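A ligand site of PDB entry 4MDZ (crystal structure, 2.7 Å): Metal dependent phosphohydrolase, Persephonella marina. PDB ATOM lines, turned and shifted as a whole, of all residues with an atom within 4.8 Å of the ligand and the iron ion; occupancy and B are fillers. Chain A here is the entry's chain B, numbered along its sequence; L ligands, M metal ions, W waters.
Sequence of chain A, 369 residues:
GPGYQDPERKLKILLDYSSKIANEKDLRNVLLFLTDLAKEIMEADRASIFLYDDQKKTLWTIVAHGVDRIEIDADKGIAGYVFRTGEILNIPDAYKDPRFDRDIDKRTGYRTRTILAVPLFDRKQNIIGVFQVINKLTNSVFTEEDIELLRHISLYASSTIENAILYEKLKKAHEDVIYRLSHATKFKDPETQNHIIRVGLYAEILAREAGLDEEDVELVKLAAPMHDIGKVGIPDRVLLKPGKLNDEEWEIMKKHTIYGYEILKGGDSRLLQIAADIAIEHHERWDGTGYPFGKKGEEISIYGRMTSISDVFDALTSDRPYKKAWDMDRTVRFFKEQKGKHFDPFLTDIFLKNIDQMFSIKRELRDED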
ATOM      1  N   HIS A 227      26.227  13.705  31.760  1.00  0.00           N
ATOM      2  CA  HIS A 227      26.325  14.689  30.662  1.00  0.00           C
ATOM      3  C   HIS A 227      27.012  15.972  31.041  1.00  0.00           C
ATOM      4  O   HIS A 227      27.713  16.552  30.209  1.00  0.00           O
ATOM      5  CB  HIS A 227      24.949  14.937  29.981  1.00  0.00           C
ATOM      6  CG  HIS A 227      23.996  15.720  30.842  1.00  0.00           C
ATOM      7  ND1 HIS A 227      23.393  15.182  31.914  1.00  0.00           N
ATOM      8  CD2 HIS A 227      23.609  17.053  30.807  1.00  0.00           C
ATOM      9  CE1 HIS A 227      22.641  16.112  32.542  1.00  0.00           C
ATOM     10  NE2 HIS A 227      22.777  17.270  31.863  1.00  0.00           N
ATOM     11  N   ASP A 228      26.854  16.422  32.293  1.00  0.00           N
ATOM     12  CA  ASP A 228      27.419  17.723  32.700  1.00  0.00           C
ATOM     13  C   ASP A 228      28.743  17.609  33.468  1.00  0.00           C
ATOM     14  O   ASP A 228      29.126  18.554  34.198  1.00  0.00           O
ATOM     15  CB  ASP A 228      26.421  18.536  33.536  1.00  0.00           C
ATOM     16  CG  ASP A 228      25.460  19.422  32.689  1.00  0.00           C
ATOM     17  OD1 ASP A 228      24.538  19.974  33.301  1.00  0.00           O
ATOM     18  OD2 ASP A 228      25.605  19.562  31.454  1.00  0.00           O
ATOM     19  N   LYS A 231      31.628  20.384  33.699  1.00  0.00           N
ATOM     20  CA  LYS A 231      31.522  21.499  34.624  1.00  0.00           C
ATOM     21  C   LYS A 231      32.648  21.568  35.643  1.00  0.00           C
ATOM     22  O   LYS A 231      33.022  22.659  36.053  1.00  0.00           O
ATOM     23  CB  LYS A 231      30.154  21.550  35.276  1.00  0.00           C
ATOM     24  CG  LYS A 231      29.049  22.012  34.321  1.00  0.00           C
ATOM     25  CD  LYS A 231      27.766  22.296  35.106  1.00  0.00           C
ATOM     26  CE  LYS A 231      26.523  22.401  34.225  1.00  0.00           C
ATOM     27  NZ  LYS A 231      25.306  22.935  34.938  1.00  0.00           N
ATOM     28  N   LYS A 241      28.721  32.501  39.188  1.00  0.00           N
ATOM     29  CA  LYS A 241      28.146  33.844  39.029  1.00  0.00           C
ATOM     30  C   LYS A 241      26.648  33.761  38.797  1.00  0.00           C
ATOM     31  O   LYS A 241      26.216  33.113  37.836  1.00  0.00           O
ATOM     32  CB  LYS A 241      28.825  34.646  37.917  1.00  0.00           C
ATOM     33  CG  LYS A 241      28.941  36.135  38.217  1.00  0.00           C
ATOM     34  CD  LYS A 241      29.394  36.911  36.986  1.00  0.00           C
ATOM     35  CE  LYS A 241      28.550  36.530  35.774  1.00  0.00           C
ATOM     36  NZ  LYS A 241      28.471  37.633  34.773  1.00  0.00           N
ATOM     37  N   PRO A 242      25.832  34.407  39.688  1.00  0.00           N
ATOM     38  CA  PRO A 242      24.375  34.269  39.525  1.00  0.00           C
ATOM     39  C   PRO A 242      23.872  35.267  38.465  1.00  0.00           C
ATOM     40  O   PRO A 242      24.489  36.326  38.235  1.00  0.00           O
ATOM     41  CB  PRO A 242      23.823  34.581  40.937  1.00  0.00           C
ATOM     42  CG  PRO A 242      24.945  35.277  41.680  1.00  0.00           C
ATOM     43  CD  PRO A 242      26.155  35.354  40.786  1.00  0.00           C
ATOM     44  N   GLY A 243      22.789  34.900  37.770  1.00  0.00           N
ATOM     45  CA  GLY A 243      22.251  35.764  36.736  1.00  0.00           C
ATOM     46  C   GLY A 243      22.996  35.679  35.423  1.00  0.00           C
ATOM     47  O   GLY A 243      23.582  34.669  35.093  1.00  0.00           O
ATOM     48  N   LYS A 244      22.997  36.773  34.684  1.00  0.00           N
ATOM     49  CA  LYS A 244      23.420  36.769  33.299  1.00  0.00           C
ATOM     50  C   LYS A 244      24.928  36.681  33.125  1.00  0.00           C
ATOM     51  O   LYS A 244      25.705  37.103  33.983  1.00  0.00           O
ATOM     52  CB  LYS A 244      22.859  38.031  32.602  1.00  0.00           C
ATOM     53  CG  LYS A 244      21.403  38.357  32.983  1.00  0.00           C
ATOM     54  CD  LYS A 244      20.459  37.170  32.744  1.00  0.00           C
ATOM     55  CE  LYS A 244      19.031  37.399  33.257  1.00  0.00           C
ATOM     56  NZ  LYS A 244      18.169  36.308  32.739  1.00  0.00           N
ATOM     57  N   LEU A 245      25.341  36.132  31.993  1.00  0.00           N
ATOM     58  CA  LEU A 245      26.747  35.998  31.693  1.00  0.00           C
ATOM     59  C   LEU A 245      27.095  36.862  30.508  1.00  0.00           C
ATOM     60  O   LEU A 245      26.361  36.896  29.530  1.00  0.00           O
ATOM     61  CB  LEU A 245      27.062  34.533  31.349  1.00  0.00           C
ATOM     62  CG  LEU A 245      27.361  33.418  32.378  1.00  0.00           C
ATOM     63  CD1 LEU A 245      28.785  33.518  32.900  1.00  0.00           C
ATOM     64  CD2 LEU A 245      26.384  33.340  33.542  1.00  0.00           C
ATOM     65  N   TRP A 250      30.070  33.154  28.859  1.00  0.00           N
ATOM     66  CA  TRP A 250      29.271  32.154  28.150  1.00  0.00           C
ATOM     67  C   TRP A 250      30.115  31.254  27.231  1.00  0.00           C
ATOM     68  O   TRP A 250      29.935  30.038  27.219  1.00  0.00           O
ATOM     69  CB  TRP A 250      28.142  32.880  27.380  1.00  0.00           C
ATOM     70  CG  TRP A 250      27.192  31.978  26.642  1.00  0.00           C
ATOM     71  CD1 TRP A 250      27.008  31.864  25.253  1.00  0.00           C
ATOM     72  CD2 TRP A 250      26.252  31.009  27.233  1.00  0.00           C
ATOM     73  NE1 TRP A 250      26.062  30.908  24.958  1.00  0.00           N
ATOM     74  CE2 TRP A 250      25.563  30.357  26.101  1.00  0.00           C
ATOM     75  CE3 TRP A 250      25.938  30.627  28.532  1.00  0.00           C
ATOM     76  CZ2 TRP A 250      24.593  29.372  26.302  1.00  0.00           C
ATOM     77  CZ3 TRP A 250      24.973  29.628  28.726  1.00  0.00           C
ATOM     78  CH2 TRP A 250      24.320  29.010  27.630  1.00  0.00           C
ATOM     79  N   MET A 253      31.535  28.877  29.481  1.00  0.00           N
ATOM     80  CA  MET A 253      30.520  27.982  30.034  1.00  0.00           C
ATOM     81  C   MET A 253      30.080  26.900  29.055  1.00  0.00           C
ATOM     82  O   MET A 253      29.897  25.741  29.462  1.00  0.00           O
ATOM     83  CB  MET A 253      29.311  28.724  30.572  1.00  0.00           C
ATOM     84  CG  MET A 253      28.250  27.786  31.139  1.00  0.00           C
ATOM     85  SD  MET A 253      28.681  26.992  32.709  1.00  0.00           S
ATOM     86  CE  MET A 253      28.041  28.221  33.856  1.00  0.00           C
ATOM     87  N   HIS A 256      32.021  23.265  28.632  1.00  0.00           N
ATOM     88  CA  HIS A 256      31.766  22.055  29.452  1.00  0.00           C
ATOM     89  C   HIS A 256      31.381  20.832  28.626  1.00  0.00           C
ATOM     90  O   HIS A 256      31.538  19.669  29.051  1.00  0.00           O
ATOM     91  CB  HIS A 256      30.725  22.321  30.521  1.00  0.00           C
ATOM     92  CG  HIS A 256      29.283  22.208  30.026  1.00  0.00           C
ATOM     93  ND1 HIS A 256      28.788  22.993  29.043  1.00  0.00           N
ATOM     94  CD2 HIS A 256      28.234  21.369  30.420  1.00  0.00           C
ATOM     95  CE1 HIS A 256      27.493  22.673  28.817  1.00  0.00           C
ATOM     96  NE2 HIS A 256      27.162  21.677  29.656  1.00  0.00           N
ATOM     97  N   HIS A 282      24.833  16.972  23.902  1.00  0.00           N
ATOM     98  CA  HIS A 282      23.524  17.279  24.438  1.00  0.00           C
ATOM     99  C   HIS A 282      23.100  18.743  24.400  1.00  0.00           C
ATOM    100  O   HIS A 282      21.976  19.068  24.827  1.00  0.00           O
ATOM    101  CB  HIS A 282      23.419  16.744  25.850  1.00  0.00           C
ATOM    102  CG  HIS A 282      24.280  17.485  26.831  1.00  0.00           C
ATOM    103  ND1 HIS A 282      25.618  17.437  26.795  1.00  0.00           N
ATOM    104  CD2 HIS A 282      23.945  18.322  27.891  1.00  0.00           C
ATOM    105  CE1 HIS A 282      26.124  18.192  27.785  1.00  0.00           C
ATOM    106  NE2 HIS A 282      25.098  18.735  28.465  1.00  0.00           N
ATOM    107  N   HIS A 283      23.962  19.636  23.930  1.00  0.00           N
ATOM    108  CA  HIS A 283      23.550  21.026  23.633  1.00  0.00           C
ATOM    109  C   HIS A 283      23.528  21.312  22.183  1.00  0.00           C
ATOM    110  O   HIS A 283      23.221  22.438  21.795  1.00  0.00           O
ATOM    111  CB  HIS A 283      24.422  22.052  24.327  1.00  0.00           C
ATOM    112  CG  HIS A 283      24.278  22.038  25.809  1.00  0.00           C
ATOM    113  ND1 HIS A 283      23.201  22.547  26.426  1.00  0.00           N
ATOM    114  CD2 HIS A 283      25.109  21.511  26.823  1.00  0.00           C
ATOM    115  CE1 HIS A 283      23.324  22.394  27.765  1.00  0.00           C
ATOM    116  NE2 HIS A 283      24.497  21.768  28.006  1.00  0.00           N
ATOM    117  N   ARG A 285      21.610  20.766  18.530  1.00  0.00           N
ATOM    118  CA  ARG A 285      20.196  20.968  18.208  1.00  0.00           C
ATOM    119  C   ARG A 285      19.929  20.395  16.825  1.00  0.00           C
ATOM    120  O   ARG A 285      20.779  20.488  15.959  1.00  0.00           O
ATOM    121  CB  ARG A 285      19.886  22.446  18.115  1.00  0.00           C
ATOM    122  CG  ARG A 285      19.543  23.131  19.418  1.00  0.00           C
ATOM    123  CD  ARG A 285      19.305  24.588  19.108  1.00  0.00           C
ATOM    124  NE  ARG A 285      19.266  25.307  20.352  1.00  0.00           N
ATOM    125  CZ  ARG A 285      18.158  25.795  20.870  1.00  0.00           C
ATOM    126  NH1 ARG A 285      17.005  25.650  20.196  1.00  0.00           N
ATOM    127  NH2 ARG A 285      18.211  26.411  22.046  1.00  0.00           N
ATOM    128  N   TYR A 291      25.285  24.669  20.161  1.00  0.00           N
ATOM    129  CA  TYR A 291      26.725  24.479  20.396  1.00  0.00           C
ATOM    130  C   TYR A 291      27.186  23.051  20.804  1.00  0.00           C
ATOM    131  O   TYR A 291      26.377  22.236  21.196  1.00  0.00           O
ATOM    132  CB  TYR A 291      27.179  25.478  21.429  1.00  0.00           C
ATOM    133  CG  TYR A 291      26.638  25.295  22.834  1.00  0.00           C
ATOM    134  CD1 TYR A 291      25.410  25.856  23.220  1.00  0.00           C
ATOM    135  CD2 TYR A 291      27.403  24.659  23.790  1.00  0.00           C
ATOM    136  CE1 TYR A 291      24.945  25.725  24.535  1.00  0.00           C
ATOM    137  CE2 TYR A 291      26.946  24.536  25.096  1.00  0.00           C
ATOM    138  CZ  TYR A 291      25.729  25.067  25.467  1.00  0.00           C
ATOM    139  OH  TYR A 291      25.334  24.917  26.761  1.00  0.00           O
ATOM    140  N   ASP A 311      17.290  16.386  29.122  1.00  0.00           N
ATOM    141  CA  ASP A 311      17.858  17.485  29.863  1.00  0.00           C
ATOM    142  C   ASP A 311      16.895  18.720  29.904  1.00  0.00           C
ATOM    143  O   ASP A 311      16.582  19.280  30.979  1.00  0.00           O
ATOM    144  CB  ASP A 311      19.237  17.827  29.287  1.00  0.00           C
ATOM    145  CG  ASP A 311      19.983  18.804  30.151  1.00  0.00           C
ATOM    146  OD1 ASP A 311      19.761  18.832  31.389  1.00  0.00           O
ATOM    147  OD2 ASP A 311      20.794  19.557  29.589  1.00  0.00           O
ATOM    148  N   VAL A 312      16.425  19.132  28.738  1.00  0.00           N
ATOM    149  CA  VAL A 312      15.504  20.250  28.678  1.00  0.00           C
ATOM    150  C   VAL A 312      14.222  19.988  29.458  1.00  0.00           C
ATOM    151  O   VAL A 312      13.754  20.861  30.167  1.00  0.00           O
ATOM    152  CB  VAL A 312      15.191  20.627  27.234  1.00  0.00           C
ATOM    153  CG1 VAL A 312      14.137  21.735  27.182  1.00  0.00           C
ATOM    154  CG2 VAL A 312      16.491  21.030  26.496  1.00  0.00           C
ATOM    155  N   ALA A 315      14.729  20.445  33.204  1.00  0.00           N
ATOM    156  CA  ALA A 315      14.995  21.807  33.619  1.00  0.00           C
ATOM    157  C   ALA A 315      13.683  22.609  33.696  1.00  0.00           C
ATOM    158  O   ALA A 315      13.410  23.328  34.671  1.00  0.00           O
ATOM    159  CB  ALA A 315      15.997  22.462  32.671  1.00  0.00           C
ATOM    160  N   LEU A 316      12.864  22.451  32.665  1.00  0.00           N
ATOM    161  CA  LEU A 316      11.658  23.223  32.513  1.00  0.00           C
ATOM    162  C   LEU A 316      10.687  22.882  33.623  1.00  0.00           C
ATOM    163  O   LEU A 316       9.805  23.702  33.938  1.00  0.00           O
ATOM    164  CB  LEU A 316      11.011  22.939  31.166  1.00  0.00           C
ATOM    165  CG  LEU A 316      11.724  23.441  29.919  1.00  0.00           C
ATOM    166  CD1 LEU A 316      10.921  22.963  28.727  1.00  0.00           C
ATOM    167  CD2 LEU A 316      11.828  24.946  29.912  1.00  0.00           C
ATOM    168  N   ARG A 320      13.460  27.429  38.701  1.00  0.00           N
ATOM    169  CA  ARG A 320      14.808  27.977  38.553  1.00  0.00           C
ATOM    170  C   ARG A 320      14.737  29.501  38.882  1.00  0.00           C
ATOM    171  O   ARG A 320      13.641  29.999  39.122  1.00  0.00           O
ATOM    172  CB  ARG A 320      15.414  27.593  37.173  1.00  0.00           C
ATOM    173  CG  ARG A 320      14.523  27.851  35.954  1.00  0.00           C
ATOM    174  CD  ARG A 320      14.494  26.697  34.945  1.00  0.00           C
ATOM    175  NE  ARG A 320      13.617  26.953  33.792  1.00  0.00           N
ATOM    176  CZ  ARG A 320      12.267  26.973  33.807  1.00  0.00           C
ATOM    177  NH1 ARG A 320      11.559  26.749  34.922  1.00  0.00           N
ATOM    178  NH2 ARG A 320      11.594  27.238  32.696  1.00  0.00           N
ATOM    179  N   LYS A 323      11.683  31.703  37.519  1.00  0.00           N
ATOM    180  CA  LYS A 323      10.713  30.900  36.744  1.00  0.00           C
ATOM    181  C   LYS A 323      10.193  29.718  37.553  1.00  0.00           C
ATOM    182  O   LYS A 323      10.965  28.883  38.022  1.00  0.00           O
ATOM    183  CB  LYS A 323      11.292  30.401  35.401  1.00  0.00           C
ATOM    184  CG  LYS A 323      12.151  31.430  34.688  1.00  0.00           C
ATOM    185  CD  LYS A 323      12.182  31.281  33.183  1.00  0.00           C
ATOM    186  CE  LYS A 323      12.618  32.599  32.556  1.00  0.00           C
ATOM    187  NZ  LYS A 323      12.909  32.458  31.109  1.00  0.00           N
ATOM    188  N   TRP A 326       7.244  24.536  34.867  1.00  0.00           N
ATOM    189  CA  TRP A 326       6.199  24.281  33.910  1.00  0.00           C
ATOM    190  C   TRP A 326       5.278  23.101  34.249  1.00  0.00           C
ATOM    191  O   TRP A 326       5.728  22.078  34.746  1.00  0.00           O
ATOM    192  CB  TRP A 326       6.916  24.062  32.563  1.00  0.00           C
ATOM    193  CG  TRP A 326       7.503  25.384  32.049  1.00  0.00           C
ATOM    194  CD1 TRP A 326       7.754  26.544  32.783  1.00  0.00           C
ATOM    195  CD2 TRP A 326       8.044  25.658  30.717  1.00  0.00           C
ATOM    196  NE1 TRP A 326       8.302  27.517  31.993  1.00  0.00           N
ATOM    197  CE2 TRP A 326       8.516  27.055  30.736  1.00  0.00           C
ATOM    198  CE3 TRP A 326       8.121  24.947  29.524  1.00  0.00           C
ATOM    199  CZ2 TRP A 326       9.055  27.674  29.607  1.00  0.00           C
ATOM    200  CZ3 TRP A 326       8.703  25.561  28.407  1.00  0.00           C
ATOM    201  CH2 TRP A 326       9.149  26.891  28.446  1.00  0.00           C
ATOM    202  N   PHE A 334       5.363  23.529  24.494  1.00  0.00           N
ATOM    203  CA  PHE A 334       6.748  23.792  24.156  1.00  0.00           C
ATOM    204  C   PHE A 334       7.413  22.696  23.273  1.00  0.00           C
ATOM    205  O   PHE A 334       7.986  23.016  22.195  1.00  0.00           O
ATOM    206  CB  PHE A 334       7.564  24.008  25.420  1.00  0.00           C
ATOM    207  CG  PHE A 334       9.034  24.128  25.173  1.00  0.00           C
ATOM    208  CD1 PHE A 334       9.599  25.328  24.748  1.00  0.00           C
ATOM    209  CD2 PHE A 334       9.892  23.018  25.361  1.00  0.00           C
ATOM    210  CE1 PHE A 334      10.992  25.436  24.523  1.00  0.00           C
ATOM    211  CE2 PHE A 334      11.279  23.118  25.135  1.00  0.00           C
ATOM    212  CZ  PHE A 334      11.831  24.325  24.727  1.00  0.00           C
ATOM    213  N   HIS A 342      14.663  22.447  18.053  1.00  0.00           N
ATOM    214  CA  HIS A 342      15.625  22.039  19.058  1.00  0.00           C
ATOM    215  C   HIS A 342      15.836  20.529  18.972  1.00  0.00           C
ATOM    216  O   HIS A 342      16.991  20.050  18.964  1.00  0.00           O
ATOM    217  CB  HIS A 342      15.102  22.465  20.424  1.00  0.00           C
ATOM    218  CG  HIS A 342      16.164  22.560  21.496  1.00  0.00           C
ATOM    219  ND1 HIS A 342      17.185  21.672  21.600  1.00  0.00           N
ATOM    220  CD2 HIS A 342      16.313  23.455  22.564  1.00  0.00           C
ATOM    221  CE1 HIS A 342      17.959  22.000  22.654  1.00  0.00           C
ATOM    222  NE2 HIS A 342      17.419  23.082  23.249  1.00  0.00           N
HETATM  223  P1  LIG L   1      19.793  24.004  32.795  1.00  0.00           P
HETATM  224  O1  LIG L   1      19.217  25.248  33.447  1.00  0.00           O
HETATM  225  O2  LIG L   1      19.407  22.657  33.365  1.00  0.00           O
HETATM  226  O3  LIG L   1      19.401  23.952  31.220  1.00  0.00           O
HETATM  227  C1  LIG L   1      19.916  23.030  30.237  1.00  0.00           C
HETATM  228  C2  LIG L   1      19.107  23.286  28.956  1.00  0.00           C
HETATM  229  O4  LIG L   1      17.734  23.418  29.338  1.00  0.00           O
HETATM  230  C3  LIG L   1      19.392  24.643  28.337  1.00  0.00           C
HETATM  231  O5  LIG L   1      20.588  24.794  27.556  1.00  0.00           O
HETATM  232  C4  LIG L   1      18.098  25.110  27.696  1.00  0.00           C
HETATM  233  O6  LIG L   1      17.833  24.676  26.361  1.00  0.00           O
HETATM  234  C5  LIG L   1      17.068  24.430  28.566  1.00  0.00           C
HETATM  235  N1  LIG L   1      16.271  25.439  29.340  1.00  0.00           N
HETATM  236  C6  LIG L   1      16.294  25.660  30.675  1.00  0.00           C
HETATM  237  N2  LIG L   1      15.400  26.628  31.022  1.00  0.00           N
HETATM  238  C7  LIG L   1      14.794  27.042  29.893  1.00  0.00           C
HETATM  239  C8  LIG L   1      13.752  28.044  29.522  1.00  0.00           C
HETATM  240  O7  LIG L   1      13.222  28.755  30.429  1.00  0.00           O
HETATM  241  N3  LIG L   1      13.396  28.166  28.219  1.00  0.00           N
HETATM  242  C9  LIG L   1      13.963  27.413  27.232  1.00  0.00           C
HETATM  243  N4  LIG L   1      13.562  27.586  25.943  1.00  0.00           N
HETATM  244  N5  LIG L   1      14.929  26.467  27.494  1.00  0.00           N
HETATM  245  C10 LIG L   1      15.364  26.248  28.776  1.00  0.00           C
HETATM  246  P2  LIG L   1      21.590  26.047  27.866  1.00  0.00           P
HETATM  247  O8  LIG L   1      20.749  27.300  27.688  1.00  0.00           O
HETATM  248  O9  LIG L   1      22.862  25.901  27.053  1.00  0.00           O
HETATM  249  O10 LIG L   1      21.944  25.933  29.448  1.00  0.00           O
HETATM  250  C11 LIG L   1      22.996  25.085  29.910  1.00  0.00           C
HETATM  251  C12 LIG L   1      23.241  25.320  31.395  1.00  0.00           C
HETATM  252  O11 LIG L   1      23.957  26.540  31.559  1.00  0.00           O
HETATM  253  C13 LIG L   1      21.961  25.446  32.228  1.00  0.00           C
HETATM  254  O12 LIG L   1      21.411  24.208  32.723  1.00  0.00           O
HETATM  255  C14 LIG L   1      22.333  26.397  33.339  1.00  0.00           C
HETATM  256  O13 LIG L   1      22.820  25.702  34.487  1.00  0.00           O
HETATM  257  C15 LIG L   1      23.446  27.234  32.713  1.00  0.00           C
HETATM  258  N6  LIG L   1      22.884  28.560  32.330  1.00  0.00           N
HETATM  259  C16 LIG L   1      22.166  28.913  31.230  1.00  0.00           C
HETATM  260  N7  LIG L   1      21.833  30.231  31.262  1.00  0.00           N
HETATM  261  C17 LIG L   1      22.329  30.767  32.408  1.00  0.00           C
HETATM  262  C18 LIG L   1      22.365  32.104  33.087  1.00  0.00           C
HETATM  263  O14 LIG L   1      21.838  33.129  32.600  1.00  0.00           O
HETATM  264  N8  LIG L   1      23.020  32.168  34.273  1.00  0.00           N
HETATM  265  C19 LIG L   1      23.634  31.104  34.870  1.00  0.00           C
HETATM  266  N9  LIG L   1      24.273  31.248  36.074  1.00  0.00           N
HETATM  267  N10 LIG L   1      23.645  29.860  34.308  1.00  0.00           N
HETATM  268  C20 LIG L   1      23.022  29.647  33.105  1.00  0.00           C
HETATM  269 FE    FE M   1      24.991  20.752  29.804  1.00  0.00          FE
HETATM  270  O   HOH W   1      19.849  22.682  25.577  1.00  0.00           O
HETATM  271  O   HOH W   2      25.952  24.286  31.889  1.00  0.00           O
HETATM  272  O   HOH W   3      26.113  25.984  29.225  1.00  0.00           O
HETATM  273  O   HOH W   4      24.097  22.042  31.458  1.00  0.00           O
HETATM  274  O   HOH W   5      17.391  20.789  35.348  1.00  0.00           O
HETATM  275  O   HOH W   6      25.421  31.091  31.663  1.00  0.00           O
HETATM  276  O   HOH W   7      11.097  29.941  27.256  1.00  0.00           O
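The iron ion is bound by a ring nitrogen (NE2) of His 283 (2.1 Å), the side-chain carboxylate (OD2) of Asp 228 (2.1 Å), water W4 (2.3 Å), a ring nitrogen (NE2) of His 256 (2.4 Å) and a ring nitrogen (NE2) of His 282 (2.4 Å).
ND1 of His 256 lies within hydrogen-bond range of O of Met 253, 3.0 Å away.
The backbone carbonyl oxygen of Leu 316 is in hydrogen-bond range of the backbone NH of Trp 326, at 2.8 Å.
NZ of Lys 241 is in hydrogen-bond range of O of Lys 244, at 2.9 Å.
OH of Tyr 291 lies within hydrogen-bond range of ND1 of His 283 (3.2 Å).
The side-chain carboxylate of Asp 228 lies within salt-bridge range of the side-chain amino group of Lys 231.
A ring nitrogen (NE2) of His 227 is in hydrogen-bond range of the side-chain carboxylate (OD1) of Asp 311 (3.4 Å).
Merely in contact with the ligand: Trp 250 (3.5 Å), Ala 315 (3.5 Å), His 342 (3.5 Å), Leu 316 (3.6 Å), Leu 245 (3.6 Å), Phe 334 (3.6 Å), Asp 311 (3.6 Å), Lys 231 (3.7 Å), Lys 323 (3.8 Å) and Val 312 (3.9 Å).
Hydrophobic or aromatic side chains within 4 Å of the ligand: Leu 245, Trp 250, His 283, Tyr 291, Val 312, Ala 315, Leu 316 and Phe 334.
Of the 24 residues printed, 15 come within 4 Å of the ligand.
Along chain A the residues within 4 Å of the ligand span positions 231 to 342.
The nearest printed residue that does not touch the ligand is Lys 244 (4.03 Å).
ND1 of His 283 lies within hydrogen-bond range of O9 of the ligand, at 3.4 Å.
NH2 of Arg 320 lies within hydrogen-bond range of O7 of the ligand (3.2 Å).
OH of Tyr 291 lies within hydrogen-bond range of O9 of the ligand (2.7 Å).
The backbone carbonyl oxygen (O) of Lys 241 sits at hydrogen-bond distance from a nitrogen (N9) of the ligand.
O of Gly 243 lies within hydrogen-bond range of N8 of the ligand (2.7 Å).
Water W1 lies within hydrogen-bond range of O6 of the ligand (2.9 Å), NE2 of His 342 (3.4 Å) and ND1 of His 283 (3.5 Å).
Water W2 bridges O11 of the ligand (3.0 Å) and NZ of Lys 231 (3.4 Å).
Water W3 lies within hydrogen-bond range of the side-chain hydroxyl (OH) of Tyr 291 (2.8 Å) and an oxygen (O11) of the ligand (3.2 Å).
Water W5 bridges an oxygen (O2) of the ligand and the backbone NH of Ala 315.
Four residues have an atom within 4 Å of the iron ion: Asp 228, His 256, His 282 and His 283.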
